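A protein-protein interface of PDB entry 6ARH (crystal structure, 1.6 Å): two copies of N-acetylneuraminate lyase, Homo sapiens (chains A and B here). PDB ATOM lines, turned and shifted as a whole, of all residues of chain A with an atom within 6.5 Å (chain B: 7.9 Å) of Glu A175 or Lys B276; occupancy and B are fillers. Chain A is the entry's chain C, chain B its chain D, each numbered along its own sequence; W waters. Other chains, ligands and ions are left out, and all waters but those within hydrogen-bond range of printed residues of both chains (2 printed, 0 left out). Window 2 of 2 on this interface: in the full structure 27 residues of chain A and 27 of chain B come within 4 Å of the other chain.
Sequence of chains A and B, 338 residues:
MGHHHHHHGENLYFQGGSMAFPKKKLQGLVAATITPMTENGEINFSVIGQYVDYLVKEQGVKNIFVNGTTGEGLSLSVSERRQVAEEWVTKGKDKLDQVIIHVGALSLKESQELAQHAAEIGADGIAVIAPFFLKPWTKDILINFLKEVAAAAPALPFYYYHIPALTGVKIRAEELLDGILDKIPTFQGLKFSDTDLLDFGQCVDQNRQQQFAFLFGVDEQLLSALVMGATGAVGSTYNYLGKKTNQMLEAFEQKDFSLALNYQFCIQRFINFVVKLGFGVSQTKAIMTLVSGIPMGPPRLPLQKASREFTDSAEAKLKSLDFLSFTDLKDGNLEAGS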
ATOM      1  N   LYS A 139       4.379  -0.203  14.973  1.00  0.00           N
ATOM      2  CA  LYS A 139       5.470  -0.626  15.843  1.00  0.00           C
ATOM      3  C   LYS A 139       5.371  -2.101  16.223  1.00  0.00           C
ATOM      4  O   LYS A 139       6.345  -2.836  16.098  1.00  0.00           O
ATOM      5  CB  LYS A 139       5.445   0.208  17.136  1.00  0.00           C
ATOM      6  CG  LYS A 139       6.360  -0.307  18.239  1.00  0.00           C
ATOM      7  CD  LYS A 139       6.140   0.451  19.535  1.00  0.00           C
ATOM      8  CE  LYS A 139       6.787  -0.267  20.695  1.00  0.00           C
ATOM      9  NZ  LYS A 139       6.764   0.584  21.914  1.00  0.00           N
ATOM     10  N   ILE A 143       8.134  -4.972  15.530  1.00  0.00           N
ATOM     11  CA  ILE A 143       8.784  -5.711  16.607  1.00  0.00           C
ATOM     12  C   ILE A 143       8.562  -7.222  16.442  1.00  0.00           C
ATOM     13  O   ILE A 143       9.465  -8.005  16.709  1.00  0.00           O
ATOM     14  CB  ILE A 143       8.305  -5.251  18.003  1.00  0.00           C
ATOM     15  CG1 ILE A 143       8.570  -3.748  18.216  1.00  0.00           C
ATOM     16  CG2 ILE A 143       8.970  -6.077  19.081  1.00  0.00           C
ATOM     17  CD1 ILE A 143      10.017  -3.338  18.211  1.00  0.00           C
ATOM     18  N   ILE A 171       8.453   5.488  12.334  1.00  0.00           N
ATOM     19  CA  ILE A 171       8.271   5.371  13.782  1.00  0.00           C
ATOM     20  C   ILE A 171       9.581   5.770  14.456  1.00  0.00           C
ATOM     21  O   ILE A 171      10.655   5.372  14.004  1.00  0.00           O
ATOM     22  CB  ILE A 171       7.908   3.938  14.216  1.00  0.00           C
ATOM     23  CG1 ILE A 171       6.625   3.456  13.519  1.00  0.00           C
ATOM     24  CG2 ILE A 171       7.732   3.862  15.737  1.00  0.00           C
ATOM     25  CD1 ILE A 171       6.654   1.973  13.234  1.00  0.00           C
ATOM     26  N   ARG A 172       9.470   6.519  15.548  1.00  0.00           N
ATOM     27  CA  ARG A 172      10.653   7.066  16.224  1.00  0.00           C
ATOM     28  C   ARG A 172      11.379   5.887  16.891  1.00  0.00           C
ATOM     29  O   ARG A 172      10.741   4.969  17.404  1.00  0.00           O
ATOM     30  CB  ARG A 172      10.289   8.132  17.262  1.00  0.00           C
ATOM     31  CG  ARG A 172       9.179   9.125  16.882  1.00  0.00           C
ATOM     32  CD  ARG A 172       9.636  10.491  16.431  1.00  0.00           C
ATOM     33  NE  ARG A 172      10.603  11.145  17.316  1.00  0.00           N
ATOM     34  CZ  ARG A 172      10.362  11.615  18.543  1.00  0.00           C
ATOM     35  NH1 ARG A 172       9.164  11.495  19.121  1.00  0.00           N
ATOM     36  NH2 ARG A 172      11.350  12.215  19.211  1.00  0.00           N
ATOM     37  N   ALA A 173      12.706   5.899  16.867  1.00  0.00           N
ATOM     38  CA  ALA A 173      13.484   4.820  17.466  1.00  0.00           C
ATOM     39  C   ALA A 173      13.225   4.690  18.959  1.00  0.00           C
ATOM     40  O   ALA A 173      13.180   3.583  19.464  1.00  0.00           O
ATOM     41  CB  ALA A 173      14.977   5.014  17.220  1.00  0.00           C
ATOM     42  N   GLU A 174      13.078   5.805  19.666  1.00  0.00           N
ATOM     43  CA  GLU A 174      12.833   5.751  21.104  1.00  0.00           C
ATOM     44  C   GLU A 174      11.527   4.984  21.397  1.00  0.00           C
ATOM     45  O   GLU A 174      11.465   4.225  22.344  1.00  0.00           O
ATOM     46  CB  GLU A 174      12.786   7.159  21.702  1.00  0.00           C
ATOM     47  CG  GLU A 174      12.648   7.189  23.231  1.00  0.00           C
ATOM     48  CD  GLU A 174      11.219   7.109  23.748  1.00  0.00           C
ATOM     49  OE1 GLU A 174      11.012   6.602  24.892  1.00  0.00           O
ATOM     50  OE2 GLU A 174      10.308   7.571  23.039  1.00  0.00           O
ATOM     51  N   GLU A 175      10.507   5.189  20.570  1.00  0.00           N
ATOM     52  CA  GLU A 175       9.233   4.471  20.715  1.00  0.00           C
ATOM     53  C   GLU A 175       9.420   2.987  20.428  1.00  0.00           C
ATOM     54  O   GLU A 175       8.922   2.147  21.158  1.00  0.00           O
ATOM     55  CB  GLU A 175       8.160   5.086  19.823  1.00  0.00           C
ATOM     56  CG  GLU A 175       7.720   6.438  20.340  1.00  0.00           C
ATOM     57  CD  GLU A 175       6.836   7.203  19.382  1.00  0.00           C
ATOM     58  OE1 GLU A 175       5.929   6.557  18.796  1.00  0.00           O
ATOM     59  OE2 GLU A 175       7.039   8.449  19.237  1.00  0.00           O
ATOM     60  N   LEU A 176      10.160   2.664  19.372  1.00  0.00           N
ATOM     61  CA  LEU A 176      10.477   1.268  19.083  1.00  0.00           C
ATOM     62  C   LEU A 176      11.208   0.570  20.234  1.00  0.00           C
ATOM     63  O   LEU A 176      10.907  -0.580  20.541  1.00  0.00           O
ATOM     64  CB  LEU A 176      11.290   1.169  17.784  1.00  0.00           C
ATOM     65  CG  LEU A 176      11.491  -0.237  17.216  1.00  0.00           C
ATOM     66  CD1 LEU A 176      11.551  -0.161  15.694  1.00  0.00           C
ATOM     67  CD2 LEU A 176      12.739  -0.945  17.745  1.00  0.00           C
ATOM     68  N   LEU A 177      12.161   1.258  20.867  1.00  0.00           N
ATOM     69  CA  LEU A 177      12.915   0.697  21.989  1.00  0.00           C
ATOM     70  C   LEU A 177      12.102   0.544  23.284  1.00  0.00           C
ATOM     71  O   LEU A 177      12.467  -0.245  24.130  1.00  0.00           O
ATOM     72  CB  LEU A 177      14.193   1.490  22.284  1.00  0.00           C
ATOM     73  CG  LEU A 177      15.463   0.986  21.574  1.00  0.00           C
ATOM     74  CD1 LEU A 177      15.239   0.785  20.081  1.00  0.00           C
ATOM     75  CD2 LEU A 177      16.599   1.955  21.865  1.00  0.00           C
ATOM     76  N   ASP A 178      11.025   1.307  23.434  1.00  0.00           N
ATOM     77  CA  ASP A 178      10.265   1.306  24.684  1.00  0.00           C
ATOM     78  C   ASP A 178       9.686  -0.083  24.939  1.00  0.00           C
ATOM     79  O   ASP A 178       8.845  -0.542  24.170  1.00  0.00           O
ATOM     80  CB  ASP A 178       9.145   2.350  24.631  1.00  0.00           C
ATOM     81  CG  ASP A 178       8.431   2.515  25.971  1.00  0.00           C
ATOM     82  OD1 ASP A 178       9.112   2.705  26.984  1.00  0.00           O
ATOM     83  OD2 ASP A 178       7.191   2.428  25.997  1.00  0.00           O
ATOM     84  N   GLY A 179      10.173  -0.755  25.981  1.00  0.00           N
ATOM     85  CA  GLY A 179       9.677  -2.087  26.338  1.00  0.00           C
ATOM     86  C   GLY A 179      10.200  -3.217  25.459  1.00  0.00           C
ATOM     87  O   GLY A 179       9.725  -4.344  25.552  1.00  0.00           O
ATOM     88  N   ASP A 199      15.161  12.337  19.081  1.00  0.00           N
ATOM     89  CA  ASP A 199      14.926  10.904  19.093  1.00  0.00           C
ATOM     90  C   ASP A 199      16.142  10.131  19.596  1.00  0.00           C
ATOM     91  O   ASP A 199      16.024   9.297  20.493  1.00  0.00           O
ATOM     92  CB  ASP A 199      14.519  10.424  17.699  1.00  0.00           C
ATOM     93  CG  ASP A 199      13.974   9.005  17.684  1.00  0.00           C
ATOM     94  OD1 ASP A 199      13.580   8.475  18.754  1.00  0.00           O
ATOM     95  OD2 ASP A 199      13.906   8.438  16.578  1.00  0.00           O
ATOM     96  N   CYS A 203      16.529   8.059  23.085  1.00  0.00           N
ATOM     97  CA  CYS A 203      16.953   6.661  23.147  1.00  0.00           C
ATOM     98  C   CYS A 203      17.950   6.461  24.276  1.00  0.00           C
ATOM     99  O   CYS A 203      17.809   5.549  25.083  1.00  0.00           O
ATOM    100  CB  CYS A 203      17.588   6.194  21.850  1.00  0.00           C
ATOM    101  SG  CYS A 203      16.385   5.953  20.540  1.00  0.00           S
ATOM    102  N   GLN A 206      16.268   7.582  27.964  1.00  0.00           N
ATOM    103  CA  GLN A 206      15.184   6.741  28.479  1.00  0.00           C
ATOM    104  C   GLN A 206      15.571   5.287  28.702  1.00  0.00           C
ATOM    105  O   GLN A 206      14.739   4.513  29.172  1.00  0.00           O
ATOM    106  CB  GLN A 206      13.975   6.807  27.534  1.00  0.00           C
ATOM    107  CG  GLN A 206      13.369   8.193  27.436  1.00  0.00           C
ATOM    108  CD  GLN A 206      12.871   8.704  28.776  1.00  0.00           C
ATOM    109  OE1 GLN A 206      12.249   7.964  29.539  1.00  0.00           O
ATOM    110  NE2 GLN A 206      13.139   9.962  29.067  1.00  0.00           N
ATOM    111  N   ARG B 269      13.015  15.819  27.657  1.00  0.00           N
ATOM    112  CA  ARG B 269      11.891  15.082  28.260  1.00  0.00           C
ATOM    113  C   ARG B 269      10.575  15.844  28.095  1.00  0.00           C
ATOM    114  O   ARG B 269       9.553  15.246  27.763  1.00  0.00           O
ATOM    115  CB  ARG B 269      12.173  14.747  29.720  1.00  0.00           C
ATOM    116  CG  ARG B 269      13.279  13.708  29.870  1.00  0.00           C
ATOM    117  CD  ARG B 269      13.562  13.363  31.326  1.00  0.00           C
ATOM    118  NE  ARG B 269      14.633  12.362  31.415  1.00  0.00           N
ATOM    119  CZ  ARG B 269      14.723  11.391  32.339  1.00  0.00           C
ATOM    120  NH1 ARG B 269      13.812  11.250  33.315  1.00  0.00           N
ATOM    121  NH2 ARG B 269      15.750  10.543  32.297  1.00  0.00           N
ATOM    122  N   PHE B 270      10.599  17.158  28.290  1.00  0.00           N
ATOM    123  CA  PHE B 270       9.400  17.958  28.092  1.00  0.00           C
ATOM    124  C   PHE B 270       9.009  18.003  26.619  1.00  0.00           C
ATOM    125  O   PHE B 270       7.870  17.702  26.264  1.00  0.00           O
ATOM    126  CB  PHE B 270       9.547  19.373  28.616  1.00  0.00           C
ATOM    127  CG  PHE B 270       8.372  20.230  28.283  1.00  0.00           C
ATOM    128  CD1 PHE B 270       7.147  19.997  28.912  1.00  0.00           C
ATOM    129  CD2 PHE B 270       8.443  21.187  27.282  1.00  0.00           C
ATOM    130  CE1 PHE B 270       6.039  20.747  28.576  1.00  0.00           C
ATOM    131  CE2 PHE B 270       7.335  21.949  26.949  1.00  0.00           C
ATOM    132  CZ  PHE B 270       6.130  21.718  27.595  1.00  0.00           C
ATOM    133  N   ILE B 271       9.955  18.387  25.765  1.00  0.00           N
ATOM    134  CA  ILE B 271       9.636  18.581  24.352  1.00  0.00           C
ATOM    135  C   ILE B 271       9.147  17.289  23.702  1.00  0.00           C
ATOM    136  O   ILE B 271       8.156  17.296  22.954  1.00  0.00           O
ATOM    137  CB  ILE B 271      10.821  19.175  23.572  1.00  0.00           C
ATOM    138  CG1 ILE B 271      11.098  20.592  24.088  1.00  0.00           C
ATOM    139  CG2 ILE B 271      10.518  19.193  22.076  1.00  0.00           C
ATOM    140  CD1 ILE B 271      12.386  21.199  23.587  1.00  0.00           C
ATOM    141  N   ASN B 272       9.810  16.170  23.997  1.00  0.00           N
ATOM    142  CA  ASN B 272       9.400  14.889  23.422  1.00  0.00           C
ATOM    143  C   ASN B 272       7.989  14.504  23.848  1.00  0.00           C
ATOM    144  O   ASN B 272       7.228  13.967  23.051  1.00  0.00           O
ATOM    145  CB  ASN B 272      10.382  13.764  23.787  1.00  0.00           C
ATOM    146  CG  ASN B 272      10.443  12.673  22.737  1.00  0.00           C
ATOM    147  OD1 ASN B 272      10.216  12.924  21.559  1.00  0.00           O
ATOM    148  ND2 ASN B 272      10.785  11.462  23.156  1.00  0.00           N
ATOM    149  N   PHE B 273       7.651  14.810  25.098  1.00  0.00           N
ATOM    150  CA  PHE B 273       6.317  14.546  25.616  1.00  0.00           C
ATOM    151  C   PHE B 273       5.273  15.287  24.773  1.00  0.00           C
ATOM    152  O   PHE B 273       4.270  14.707  24.382  1.00  0.00           O
ATOM    153  CB  PHE B 273       6.261  14.949  27.087  1.00  0.00           C
ATOM    154  CG  PHE B 273       4.950  14.662  27.752  1.00  0.00           C
ATOM    155  CD1 PHE B 273       4.714  13.432  28.376  1.00  0.00           C
ATOM    156  CD2 PHE B 273       3.964  15.628  27.766  1.00  0.00           C
ATOM    157  CE1 PHE B 273       3.501  13.180  29.010  1.00  0.00           C
ATOM    158  CE2 PHE B 273       2.748  15.384  28.383  1.00  0.00           C
ATOM    159  CZ  PHE B 273       2.516  14.160  29.007  1.00  0.00           C
ATOM    160  N   VAL B 274       5.526  16.553  24.469  1.00  0.00           N
ATOM    161  CA  VAL B 274       4.567  17.327  23.680  1.00  0.00           C
ATOM    162  C   VAL B 274       4.605  16.983  22.192  1.00  0.00           C
ATOM    163  O   VAL B 274       3.551  16.983  21.554  1.00  0.00           O
ATOM    164  CB  VAL B 274       4.606  18.846  23.971  1.00  0.00           C
ATOM    165  CG1 VAL B 274       4.170  19.094  25.413  1.00  0.00           C
ATOM    166  CG2 VAL B 274       5.960  19.456  23.716  1.00  0.00           C
ATOM    167  N   VAL B 275       5.789  16.661  21.663  1.00  0.00           N
ATOM    168  CA  VAL B 275       5.930  16.189  20.273  1.00  0.00           C
ATOM    169  C   VAL B 275       5.026  14.968  20.026  1.00  0.00           C
ATOM    170  O   VAL B 275       4.310  14.915  19.021  1.00  0.00           O
ATOM    171  CB  VAL B 275       7.405  15.888  19.904  1.00  0.00           C
ATOM    172  CG1 VAL B 275       7.504  15.051  18.617  1.00  0.00           C
ATOM    173  CG2 VAL B 275       8.197  17.197  19.750  1.00  0.00           C
ATOM    174  N   LYS B 276       5.032  14.017  20.948  1.00  0.00           N
ATOM    175  CA  LYS B 276       4.134  12.848  20.833  1.00  0.00           C
ATOM    176  C   LYS B 276       2.633  13.188  20.797  1.00  0.00           C
ATOM    177  O   LYS B 276       1.868  12.493  20.136  1.00  0.00           O
ATOM    178  CB  LYS B 276       4.415  11.847  21.953  1.00  0.00           C
ATOM    179  CG  LYS B 276       5.769  11.184  21.831  1.00  0.00           C
ATOM    180  CD  LYS B 276       6.154  10.487  23.110  1.00  0.00           C
ATOM    181  CE  LYS B 276       7.475   9.767  22.928  1.00  0.00           C
ATOM    182  NZ  LYS B 276       7.937   9.191  24.207  1.00  0.00           N
ATOM    183  N   LEU B 277       2.217  14.242  21.498  1.00  0.00           N
ATOM    184  CA  LEU B 277       0.811  14.670  21.540  1.00  0.00           C
ATOM    185  C   LEU B 277       0.363  15.493  20.333  1.00  0.00           C
ATOM    186  O   LEU B 277      -0.823  15.508  20.013  1.00  0.00           O
ATOM    187  CB  LEU B 277       0.532  15.479  22.808  1.00  0.00           C
ATOM    188  CG  LEU B 277       0.731  14.795  24.156  1.00  0.00           C
ATOM    189  CD1 LEU B 277       0.543  15.798  25.281  1.00  0.00           C
ATOM    190  CD2 LEU B 277      -0.234  13.626  24.310  1.00  0.00           C
ATOM    191  N   GLY B 278       1.302  16.170  19.678  1.00  0.00           N
ATOM    192  CA  GLY B 278       0.990  17.130  18.618  1.00  0.00           C
ATOM    193  C   GLY B 278       1.439  18.499  19.087  1.00  0.00           C
ATOM    194  O   GLY B 278       0.738  19.138  19.863  1.00  0.00           O
ATOM    195  N   PHE B 279       2.611  18.922  18.625  1.00  0.00           N
ATOM    196  CA  PHE B 279       3.264  20.135  19.110  1.00  0.00           C
ATOM    197  C   PHE B 279       3.561  21.114  17.981  1.00  0.00           C
ATOM    198  O   PHE B 279       4.542  20.989  17.255  1.00  0.00           O
ATOM    199  CB  PHE B 279       4.554  19.772  19.826  1.00  0.00           C
ATOM    200  CG  PHE B 279       5.262  20.938  20.449  1.00  0.00           C
ATOM    201  CD1 PHE B 279       4.594  21.797  21.318  1.00  0.00           C
ATOM    202  CD2 PHE B 279       6.610  21.145  20.212  1.00  0.00           C
ATOM    203  CE1 PHE B 279       5.259  22.861  21.908  1.00  0.00           C
ATOM    204  CE2 PHE B 279       7.281  22.202  20.804  1.00  0.00           C
ATOM    205  CZ  PHE B 279       6.603  23.057  21.654  1.00  0.00           C
ATOM    206  N   PHE B 310      -4.564  19.053  26.597  1.00  0.00           N
ATOM    207  CA  PHE B 310      -3.153  19.296  26.285  1.00  0.00           C
ATOM    208  C   PHE B 310      -2.502  20.196  27.327  1.00  0.00           C
ATOM    209  O   PHE B 310      -1.431  19.877  27.845  1.00  0.00           O
ATOM    210  CB  PHE B 310      -2.962  19.900  24.885  1.00  0.00           C
ATOM    211  CG  PHE B 310      -1.543  20.278  24.621  1.00  0.00           C
ATOM    212  CD1 PHE B 310      -0.633  19.334  24.124  1.00  0.00           C
ATOM    213  CD2 PHE B 310      -1.087  21.544  24.936  1.00  0.00           C
ATOM    214  CE1 PHE B 310       0.702  19.672  23.924  1.00  0.00           C
ATOM    215  CE2 PHE B 310       0.250  21.887  24.756  1.00  0.00           C
ATOM    216  CZ  PHE B 310       1.144  20.949  24.258  1.00  0.00           C
HETATM  217  O   HOH W   1       8.230   5.716  24.140  1.00  0.00           O
HETATM  218  O   HOH W   2       9.889   8.690  26.378  1.00  0.00           O
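The guanidinium group (NH2) of Arg A172 lies within hydrogen-bond range of the side-chain amide oxygen (OD1) of Asn B272.
The side-chain carboxylate of Glu A174 lies within salt-bridge range of the side-chain amino group of Lys B276, at 3.1 Å.
The side-chain amino group (NZ) of Lys A139 sits at hydrogen-bond distance from the backbone carbonyl oxygen (O) of Glu A175.
OE2 of Glu A175 is in salt-bridge range of NH1 of Arg A172, 3.7 Å away.
The backbone NH (N) of Glu A174 lies within hydrogen-bond range of the side-chain carboxylate (OD1) of Asp A199 (2.9 Å).
The backbone NH of Glu A174 lies within hydrogen-bond range of the side-chain sulfur of Cys A203, 3.4 Å away.
Val B275 touches Arg A172 (CG1 to NH1, 3.96 Å).
ND2 of Asn B272 touches OE2 of Glu A174, at 3.9 Å.
Lys B276 touches Glu A175.
NE2 of Gln A206 touches NE of Arg B269 (3.7 Å).
Glu A175 touches just one residue of chain B: Lys B276.
Lys B276 touches just these residues of chain A: Glu A174 and Glu A175.
Of the printed residues of chain B, Glu A174 touches Asn B272 and Lys B276.
Printed residues of chain B within 4 Å of Arg A172: Asn B272 and Val B275.
Of the printed residues of chain B, Gln A206 touches Arg B269 (3.7 Å).
Printed residues of chain A within 4 Å of Val B275: Arg A172.
Of the printed residues of chain A, Arg B269 touches Gln A206.
Cys A203 touches none of the printed residues of chain B.
Leu B277 touches none of the printed residues of chain A.
Hydrophobic or aromatic side chains of chain B that line the printed part of chain A: Val B275.
Among the printed residues, Asp or Glu carboxylates within 4 Å of a Lys or Arg side-chain nitrogen of the other chain: Glu A174 with Lys B276 (3.1 Å).
No position is printed for both chains.
Water W2 lies within hydrogen-bond range of OE1 of Glu A174 (2.8 Å) and NZ of Lys B276 (3.0 Å).
Water W1 bridges the side-chain carboxylate of Glu A174 (3.0 Å) and the side-chain amino group of Lys B276 (3.5 Å).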
